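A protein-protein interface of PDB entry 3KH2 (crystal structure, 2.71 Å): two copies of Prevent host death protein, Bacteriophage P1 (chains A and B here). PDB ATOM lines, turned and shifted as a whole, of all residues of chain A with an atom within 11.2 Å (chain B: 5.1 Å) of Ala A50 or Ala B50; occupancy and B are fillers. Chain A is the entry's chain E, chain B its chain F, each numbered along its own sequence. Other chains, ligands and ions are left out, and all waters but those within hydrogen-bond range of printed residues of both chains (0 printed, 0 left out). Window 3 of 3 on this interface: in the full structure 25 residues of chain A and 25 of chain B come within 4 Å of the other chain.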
ATOM      1  N   LYS A  41      11.107  18.578  -5.646  1.00  0.00           N
ATOM      2  CA  LYS A  41      10.906  17.745  -6.830  1.00  0.00           C
ATOM      3  C   LYS A  41      12.040  16.734  -6.984  1.00  0.00           C
ATOM      4  O   LYS A  41      11.818  15.612  -7.437  1.00  0.00           O
ATOM      5  CB  LYS A  41      10.800  18.604  -8.094  1.00  0.00           C
ATOM      6  CG  LYS A  41      10.240  17.849  -9.297  1.00  0.00           C
ATOM      7  CD  LYS A  41      10.472  18.586 -10.605  1.00  0.00           C
ATOM      8  CE  LYS A  41      10.061  17.727 -11.789  1.00  0.00           C
ATOM      9  NZ  LYS A  41      10.098  18.477 -13.071  1.00  0.00           N
ATOM     10  N   ALA A  42      13.247  17.137  -6.602  1.00  0.00           N
ATOM     11  CA  ALA A  42      14.420  16.277  -6.694  1.00  0.00           C
ATOM     12  C   ALA A  42      14.263  15.010  -5.858  1.00  0.00           C
ATOM     13  O   ALA A  42      14.510  13.908  -6.354  1.00  0.00           O
ATOM     14  CB  ALA A  42      15.666  17.033  -6.266  1.00  0.00           C
ATOM     15  N   THR A  43      13.858  15.172  -4.597  1.00  0.00           N
ATOM     16  CA  THR A  43      13.714  14.029  -3.684  1.00  0.00           C
ATOM     17  C   THR A  43      12.443  13.238  -3.991  1.00  0.00           C
ATOM     18  O   THR A  43      12.464  12.007  -3.966  1.00  0.00           O
ATOM     19  CB  THR A  43      13.768  14.425  -2.165  1.00  0.00           C
ATOM     20  OG1 THR A  43      13.111  15.675  -1.947  1.00  0.00           O
ATOM     21  CG2 THR A  43      15.209  14.536  -1.678  1.00  0.00           C
ATOM     22  N   PHE A  44      11.349  13.935  -4.295  1.00  0.00           N
ATOM     23  CA  PHE A  44      10.109  13.259  -4.692  1.00  0.00           C
ATOM     24  C   PHE A  44      10.338  12.343  -5.897  1.00  0.00           C
ATOM     25  O   PHE A  44       9.964  11.179  -5.870  1.00  0.00           O
ATOM     26  CB  PHE A  44       8.992  14.265  -5.004  1.00  0.00           C
ATOM     27  CG  PHE A  44       7.696  13.619  -5.429  1.00  0.00           C
ATOM     28  CD1 PHE A  44       6.725  13.305  -4.494  1.00  0.00           C
ATOM     29  CD2 PHE A  44       7.453  13.316  -6.768  1.00  0.00           C
ATOM     30  CE1 PHE A  44       5.532  12.704  -4.886  1.00  0.00           C
ATOM     31  CE2 PHE A  44       6.264  12.712  -7.165  1.00  0.00           C
ATOM     32  CZ  PHE A  44       5.305  12.407  -6.223  1.00  0.00           C
ATOM     33  N   GLU A  45      10.960  12.871  -6.944  1.00  0.00           N
ATOM     34  CA  GLU A  45      11.207  12.098  -8.163  1.00  0.00           C
ATOM     35  C   GLU A  45      12.104  10.888  -7.910  1.00  0.00           C
ATOM     36  O   GLU A  45      11.921   9.843  -8.524  1.00  0.00           O
ATOM     37  CB  GLU A  45      11.828  12.978  -9.251  1.00  0.00           C
ATOM     38  CG  GLU A  45      10.873  14.008  -9.860  1.00  0.00           C
ATOM     39  CD  GLU A  45      10.098  13.481 -11.064  1.00  0.00           C
ATOM     40  OE1 GLU A  45       9.540  12.361 -10.986  1.00  0.00           O
ATOM     41  OE2 GLU A  45      10.042  14.197 -12.091  1.00  0.00           O
ATOM     42  N   ALA A  46      13.070  11.038  -7.009  1.00  0.00           N
ATOM     43  CA  ALA A  46      13.967   9.944  -6.646  1.00  0.00           C
ATOM     44  C   ALA A  46      13.206   8.848  -5.911  1.00  0.00           C
ATOM     45  O   ALA A  46      13.470   7.666  -6.106  1.00  0.00           O
ATOM     46  CB  ALA A  46      15.124  10.455  -5.797  1.00  0.00           C
ATOM     47  N   TYR A  47      12.259   9.246  -5.070  1.00  0.00           N
ATOM     48  CA  TYR A  47      11.417   8.290  -4.357  1.00  0.00           C
ATOM     49  C   TYR A  47      10.504   7.552  -5.314  1.00  0.00           C
ATOM     50  O   TYR A  47      10.376   6.337  -5.233  1.00  0.00           O
ATOM     51  CB  TYR A  47      10.575   8.982  -3.277  1.00  0.00           C
ATOM     52  CG  TYR A  47      11.338   9.463  -2.063  1.00  0.00           C
ATOM     53  CD1 TYR A  47      12.584   8.937  -1.728  1.00  0.00           C
ATOM     54  CD2 TYR A  47      10.790  10.421  -1.226  1.00  0.00           C
ATOM     55  CE1 TYR A  47      13.271   9.378  -0.613  1.00  0.00           C
ATOM     56  CE2 TYR A  47      11.469  10.867  -0.103  1.00  0.00           C
ATOM     57  CZ  TYR A  47      12.707  10.341   0.198  1.00  0.00           C
ATOM     58  OH  TYR A  47      13.381  10.772   1.311  1.00  0.00           O
ATOM     59  N   LYS A  48       9.874   8.302  -6.211  1.00  0.00           N
ATOM     60  CA  LYS A  48       9.020   7.739  -7.265  1.00  0.00           C
ATOM     61  C   LYS A  48       9.772   6.714  -8.115  1.00  0.00           C
ATOM     62  O   LYS A  48       9.238   5.660  -8.453  1.00  0.00           O
ATOM     63  CB  LYS A  48       8.488   8.863  -8.159  1.00  0.00           C
ATOM     64  CG  LYS A  48       7.295   8.496  -9.033  1.00  0.00           C
ATOM     65  CD  LYS A  48       7.000   9.620 -10.029  1.00  0.00           C
ATOM     66  CE  LYS A  48       5.765   9.341 -10.881  1.00  0.00           C
ATOM     67  NZ  LYS A  48       4.495   9.554 -10.119  1.00  0.00           N
ATOM     68  N   LYS A  49      11.018   7.033  -8.447  1.00  0.00           N
ATOM     69  CA  LYS A  49      11.847   6.176  -9.290  1.00  0.00           C
ATOM     70  C   LYS A  49      12.167   4.843  -8.607  1.00  0.00           C
ATOM     71  O   LYS A  49      12.196   3.797  -9.257  1.00  0.00           O
ATOM     72  CB  LYS A  49      13.126   6.920  -9.685  1.00  0.00           C
ATOM     73  CG  LYS A  49      14.073   6.160 -10.617  1.00  0.00           C
ATOM     74  CD  LYS A  49      15.407   5.805  -9.927  1.00  0.00           C
ATOM     75  CE  LYS A  49      16.555   5.601 -10.929  1.00  0.00           C
ATOM     76  NZ  LYS A  49      16.225   4.610 -11.985  1.00  0.00           N
ATOM     77  N   ALA A  50      12.406   4.894  -7.301  1.00  0.00           N
ATOM     78  CA  ALA A  50      12.657   3.694  -6.511  1.00  0.00           C
ATOM     79  C   ALA A  50      11.401   2.828  -6.460  1.00  0.00           C
ATOM     80  O   ALA A  50      11.476   1.602  -6.570  1.00  0.00           O
ATOM     81  CB  ALA A  50      13.101   4.070  -5.107  1.00  0.00           C
ATOM     82  N   ALA A  51      10.249   3.473  -6.291  1.00  0.00           N
ATOM     83  CA  ALA A  51       8.957   2.785  -6.353  1.00  0.00           C
ATOM     84  C   ALA A  51       8.810   2.056  -7.689  1.00  0.00           C
ATOM     85  O   ALA A  51       8.423   0.892  -7.725  1.00  0.00           O
ATOM     86  CB  ALA A  51       7.823   3.774  -6.163  1.00  0.00           C
ATOM     87  N   LEU A  52       9.150   2.753  -8.774  1.00  0.00           N
ATOM     88  CA  LEU A  52       9.105   2.213 -10.134  1.00  0.00           C
ATOM     89  C   LEU A  52      10.071   1.047 -10.361  1.00  0.00           C
ATOM     90  O   LEU A  52       9.721   0.080 -11.031  1.00  0.00           O
ATOM     91  CB  LEU A  52       9.404   3.336 -11.137  1.00  0.00           C
ATOM     92  CG  LEU A  52       9.103   3.111 -12.618  1.00  0.00           C
ATOM     93  CD1 LEU A  52       7.613   2.994 -12.845  1.00  0.00           C
ATOM     94  CD2 LEU A  52       9.683   4.256 -13.429  1.00  0.00           C
ATOM     95  N   ASP A  53      11.286   1.147  -9.824  1.00  0.00           N
ATOM     96  CA  ASP A  53      12.288   0.080  -9.953  1.00  0.00           C
ATOM     97  C   ASP A  53      11.767  -1.225  -9.365  1.00  0.00           C
ATOM     98  O   ASP A  53      11.871  -2.286  -9.983  1.00  0.00           O
ATOM     99  CB  ASP A  53      13.588   0.472  -9.247  1.00  0.00           C
ATOM    100  CG  ASP A  53      14.354   1.564  -9.978  1.00  0.00           C
ATOM    101  OD1 ASP A  53      14.127   1.744 -11.199  1.00  0.00           O
ATOM    102  OD2 ASP A  53      15.201   2.233  -9.333  1.00  0.00           O
ATOM    103  N   ALA A  54      11.208  -1.126  -8.161  1.00  0.00           N
ATOM    104  CA  ALA A  54      10.576  -2.255  -7.483  1.00  0.00           C
ATOM    105  C   ALA A  54       9.399  -2.811  -8.287  1.00  0.00           C
ATOM    106  O   ALA A  54       9.159  -4.015  -8.298  1.00  0.00           O
ATOM    107  CB  ALA A  54      10.107  -1.833  -6.109  1.00  0.00           C
ATOM    108  N   GLU A  55       8.673  -1.919  -8.953  1.00  0.00           N
ATOM    109  CA  GLU A  55       7.538  -2.293  -9.784  1.00  0.00           C
ATOM    110  C   GLU A  55       7.985  -3.131 -10.982  1.00  0.00           C
ATOM    111  O   GLU A  55       7.335  -4.118 -11.323  1.00  0.00           O
ATOM    112  CB  GLU A  55       6.774  -1.043 -10.254  1.00  0.00           C
ATOM    113  CG  GLU A  55       5.373  -1.347 -10.803  1.00  0.00           C
ATOM    114  CD  GLU A  55       4.555  -0.102 -11.160  1.00  0.00           C
ATOM    115  OE1 GLU A  55       4.961   1.036 -10.824  1.00  0.00           O
ATOM    116  OE2 GLU A  55       3.486  -0.267 -11.784  1.00  0.00           O
ATOM    117  N   PHE A  56       9.094  -2.743 -11.612  1.00  0.00           N
ATOM    118  CA  PHE A  56       9.647  -3.511 -12.740  1.00  0.00           C
ATOM    119  C   PHE A  56      10.247  -4.824 -12.277  1.00  0.00           C
ATOM    120  O   PHE A  56      10.203  -5.812 -13.001  1.00  0.00           O
ATOM    121  CB  PHE A  56      10.738  -2.728 -13.494  1.00  0.00           C
ATOM    122  CG  PHE A  56      10.256  -1.463 -14.167  1.00  0.00           C
ATOM    123  CD1 PHE A  56       8.932  -1.301 -14.564  1.00  0.00           C
ATOM    124  CD2 PHE A  56      11.155  -0.437 -14.438  1.00  0.00           C
ATOM    125  CE1 PHE A  56       8.513  -0.134 -15.190  1.00  0.00           C
ATOM    126  CE2 PHE A  56      10.739   0.738 -15.075  1.00  0.00           C
ATOM    127  CZ  PHE A  56       9.417   0.889 -15.450  1.00  0.00           C
ATOM    128  N   ALA A  57      10.825  -4.828 -11.081  1.00  0.00           N
ATOM    129  CA  ALA A  57      11.624  -5.959 -10.629  1.00  0.00           C
ATOM    130  C   ALA A  57      10.753  -7.175 -10.354  1.00  0.00           C
ATOM    131  O   ALA A  57      11.174  -8.309 -10.579  1.00  0.00           O
ATOM    132  CB  ALA A  57      12.425  -5.589  -9.406  1.00  0.00           C
ATOM    133  N   SER A  58       9.535  -6.932  -9.882  1.00  0.00           N
ATOM    134  CA  SER A  58       8.602  -8.011  -9.579  1.00  0.00           C
ATOM    135  C   SER A  58       7.856  -8.495 -10.819  1.00  0.00           C
ATOM    136  O   SER A  58       7.460  -9.655 -10.881  1.00  0.00           O
ATOM    137  CB  SER A  58       7.614  -7.580  -8.497  1.00  0.00           C
ATOM    138  OG  SER A  58       6.916  -6.426  -8.886  1.00  0.00           O
ATOM    139  N   ALA B  46       4.672   5.809   0.686  1.00  0.00           N
ATOM    140  CA  ALA B  46       4.879   4.552  -0.027  1.00  0.00           C
ATOM    141  C   ALA B  46       6.112   4.647  -0.922  1.00  0.00           C
ATOM    142  O   ALA B  46       6.851   3.680  -1.053  1.00  0.00           O
ATOM    143  CB  ALA B  46       3.650   4.181  -0.838  1.00  0.00           C
ATOM    144  N   TYR B  47       6.330   5.810  -1.529  1.00  0.00           N
ATOM    145  CA  TYR B  47       7.517   6.035  -2.351  1.00  0.00           C
ATOM    146  C   TYR B  47       8.768   6.158  -1.485  1.00  0.00           C
ATOM    147  O   TYR B  47       9.820   5.636  -1.842  1.00  0.00           O
ATOM    148  CB  TYR B  47       7.374   7.288  -3.223  1.00  0.00           C
ATOM    149  CG  TYR B  47       6.329   7.240  -4.335  1.00  0.00           C
ATOM    150  CD1 TYR B  47       5.761   6.039  -4.762  1.00  0.00           C
ATOM    151  CD2 TYR B  47       5.943   8.410  -4.989  1.00  0.00           C
ATOM    152  CE1 TYR B  47       4.819   6.018  -5.782  1.00  0.00           C
ATOM    153  CE2 TYR B  47       5.007   8.394  -6.013  1.00  0.00           C
ATOM    154  CZ  TYR B  47       4.450   7.198  -6.401  1.00  0.00           C
ATOM    155  OH  TYR B  47       3.526   7.175  -7.412  1.00  0.00           O
ATOM    156  N   LYS B  48       8.653   6.841  -0.351  1.00  0.00           N
ATOM    157  CA  LYS B  48       9.763   6.961   0.612  1.00  0.00           C
ATOM    158  C   LYS B  48      10.254   5.604   1.127  1.00  0.00           C
ATOM    159  O   LYS B  48      11.439   5.433   1.410  1.00  0.00           O
ATOM    160  CB  LYS B  48       9.334   7.824   1.796  1.00  0.00           C
ATOM    161  CG  LYS B  48      10.464   8.344   2.656  1.00  0.00           C
ATOM    162  CD  LYS B  48       9.922   9.258   3.761  1.00  0.00           C
ATOM    163  CE  LYS B  48      11.022   9.773   4.677  1.00  0.00           C
ATOM    164  NZ  LYS B  48      11.900  10.756   3.987  1.00  0.00           N
ATOM    165  N   LYS B  49       9.333   4.650   1.248  1.00  0.00           N
ATOM    166  CA  LYS B  49       9.652   3.320   1.773  1.00  0.00           C
ATOM    167  C   LYS B  49      10.318   2.450   0.721  1.00  0.00           C
ATOM    168  O   LYS B  49      11.179   1.633   1.037  1.00  0.00           O
ATOM    169  CB  LYS B  49       8.393   2.628   2.292  1.00  0.00           C
ATOM    170  CG  LYS B  49       8.604   1.168   2.701  1.00  0.00           C
ATOM    171  CD  LYS B  49       7.385   0.616   3.424  1.00  0.00           C
ATOM    172  CE  LYS B  49       7.347  -0.915   3.393  1.00  0.00           C
ATOM    173  NZ  LYS B  49       8.685  -1.540   3.616  1.00  0.00           N
ATOM    174  N   ALA B  50       9.898   2.611  -0.525  1.00  0.00           N
ATOM    175  CA  ALA B  50      10.551   1.951  -1.640  1.00  0.00           C
ATOM    176  C   ALA B  50      12.014   2.373  -1.699  1.00  0.00           C
ATOM    177  O   ALA B  50      12.898   1.533  -1.879  1.00  0.00           O
ATOM    178  CB  ALA B  50       9.852   2.288  -2.934  1.00  0.00           C
ATOM    179  N   ALA B  51      12.262   3.673  -1.526  1.00  0.00           N
ATOM    180  CA  ALA B  51      13.619   4.232  -1.615  1.00  0.00           C
ATOM    181  C   ALA B  51      14.499   3.721  -0.484  1.00  0.00           C
ATOM    182  O   ALA B  51      15.608   3.238  -0.714  1.00  0.00           O
ATOM    183  CB  ALA B  51      13.572   5.742  -1.603  1.00  0.00           C
ATOM    184  N   LEU B  52      13.984   3.826   0.736  1.00  0.00           N
ATOM    185  CA  LEU B  52      14.659   3.297   1.920  1.00  0.00           C
ATOM    186  C   LEU B  52      14.945   1.796   1.796  1.00  0.00           C
ATOM    187  O   LEU B  52      16.054   1.346   2.096  1.00  0.00           O
ATOM    188  CB  LEU B  52      13.816   3.566   3.166  1.00  0.00           C
ATOM    189  CG  LEU B  52      14.522   3.375   4.506  1.00  0.00           C
ATOM    190  CD1 LEU B  52      15.751   4.265   4.608  1.00  0.00           C
ATOM    191  CD2 LEU B  52      13.551   3.656   5.646  1.00  0.00           C
ATOM    192  N   ASP B  53      13.946   1.025   1.358  1.00  0.00           N
ATOM    193  CA  ASP B  53      14.130  -0.411   1.138  1.00  0.00           C
ATOM    194  C   ASP B  53      15.262  -0.674   0.155  1.00  0.00           C
ATOM    195  O   ASP B  53      16.037  -1.604   0.349  1.00  0.00           O
ATOM    196  CB  ASP B  53      12.843  -1.078   0.629  1.00  0.00           C
ATOM    197  CG  ASP B  53      11.808  -1.315   1.739  1.00  0.00           C
ATOM    198  OD1 ASP B  53      12.120  -1.055   2.923  1.00  0.00           O
ATOM    199  OD2 ASP B  53      10.676  -1.767   1.426  1.00  0.00           O
ATOM    200  N   ALA B  54      15.354   0.142  -0.892  1.00  0.00           N
ATOM    201  CA  ALA B  54      16.377  -0.041  -1.934  1.00  0.00           C
ATOM    202  C   ALA B  54      17.754   0.263  -1.367  1.00  0.00           C
ATOM    203  O   ALA B  54      18.739  -0.427  -1.664  1.00  0.00           O
ATOM    204  CB  ALA B  54      16.093   0.858  -3.123  1.00  0.00           C
ATOM    205  N   GLU B  55      17.788   1.309  -0.546  1.00  0.00           N
ATOM    206  CA  GLU B  55      18.992   1.774   0.130  1.00  0.00           C
ATOM    207  C   GLU B  55      19.571   0.653   0.991  1.00  0.00           C
ATOM    208  O   GLU B  55      20.772   0.387   0.948  1.00  0.00           O
ATOM    209  CB  GLU B  55      18.651   3.013   0.981  1.00  0.00           C
ATOM    210  CG  GLU B  55      19.847   3.827   1.477  1.00  0.00           C
ATOM    211  CD  GLU B  55      19.442   5.107   2.236  1.00  0.00           C
ATOM    212  OE1 GLU B  55      18.227   5.370   2.429  1.00  0.00           O
ATOM    213  OE2 GLU B  55      20.358   5.858   2.643  1.00  0.00           O
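The side-chain hydroxyl of Tyr A47 sits at hydrogen-bond distance from the side-chain amino group of Lys B48, 3.1 Å away.
Among the printed residues, merely in contact across the chains: Tyr A47 with Tyr B47, Tyr A47 with Ala B51, Lys A48 with Tyr B47, Ala A50 with Ala B50, Ala A50 with Ala B51, Ala A51 with Tyr B47 and Ala A51 with Ala B50.
Of chain B, only Ala B50 (3.9 Å) and Ala B51 (3.5 Å) come within 4 Å of Ala A50. Printed residues of chain A within 4 Å of Ala B50: Ala A50 (3.9 Å) and Ala A51 (3.6 Å). Ala B46 touches none of the printed residues of chain A. No residue of chain A comes within 4 Å of Lys B49. Ala B51 touches just these residues of chain A: Tyr A47 (3.3 Å) and Ala A50 (3.5 Å). No residue of chain A comes within 4 Å of Asp B53. Of the printed residues of chain B, Lys A48 touches Tyr B47. Of the printed residues of chain B, Ala A51 touches Tyr B47 (3.4 Å) and Ala B50 (3.6 Å). Printed residues of chain B within 4 Å of Tyr A47: Tyr B47, Lys B48 and Ala B51. Of the printed residues of chain A, Tyr B47 touches Tyr A47, Lys A48 and Ala A51. Of the printed residues of chain A, Lys B48 touches Tyr A47. Lys A49 touches none of the printed residues of chain B. Ala A46 touches none of the printed residues of chain B. The nearest residue of chain B that does not touch Ala A50 is Ala B54 (4.8 Å). The nearest residue of chain A that does not touch Ala B50 is Tyr A47 (4.7 Å). The nearest printed residue of chain A that does not touch Lys B48 is Lys A48 (6.2 Å).
Tyr B47 touches its own counterpart, Tyr A47. Tyr A47 touches Lys B48, and with the chains exchanged Lys A48 touches Tyr B47. Tyr A47 touches Ala B51, and with the chains exchanged Ala A51 touches Tyr B47. Ala A50 touches Ala B51, and with the chains exchanged Ala A51 touches Ala B50. Of the 8 pairs that touch across the chains among the printed residues, 8 have their exchanged pair printed and touching as well.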
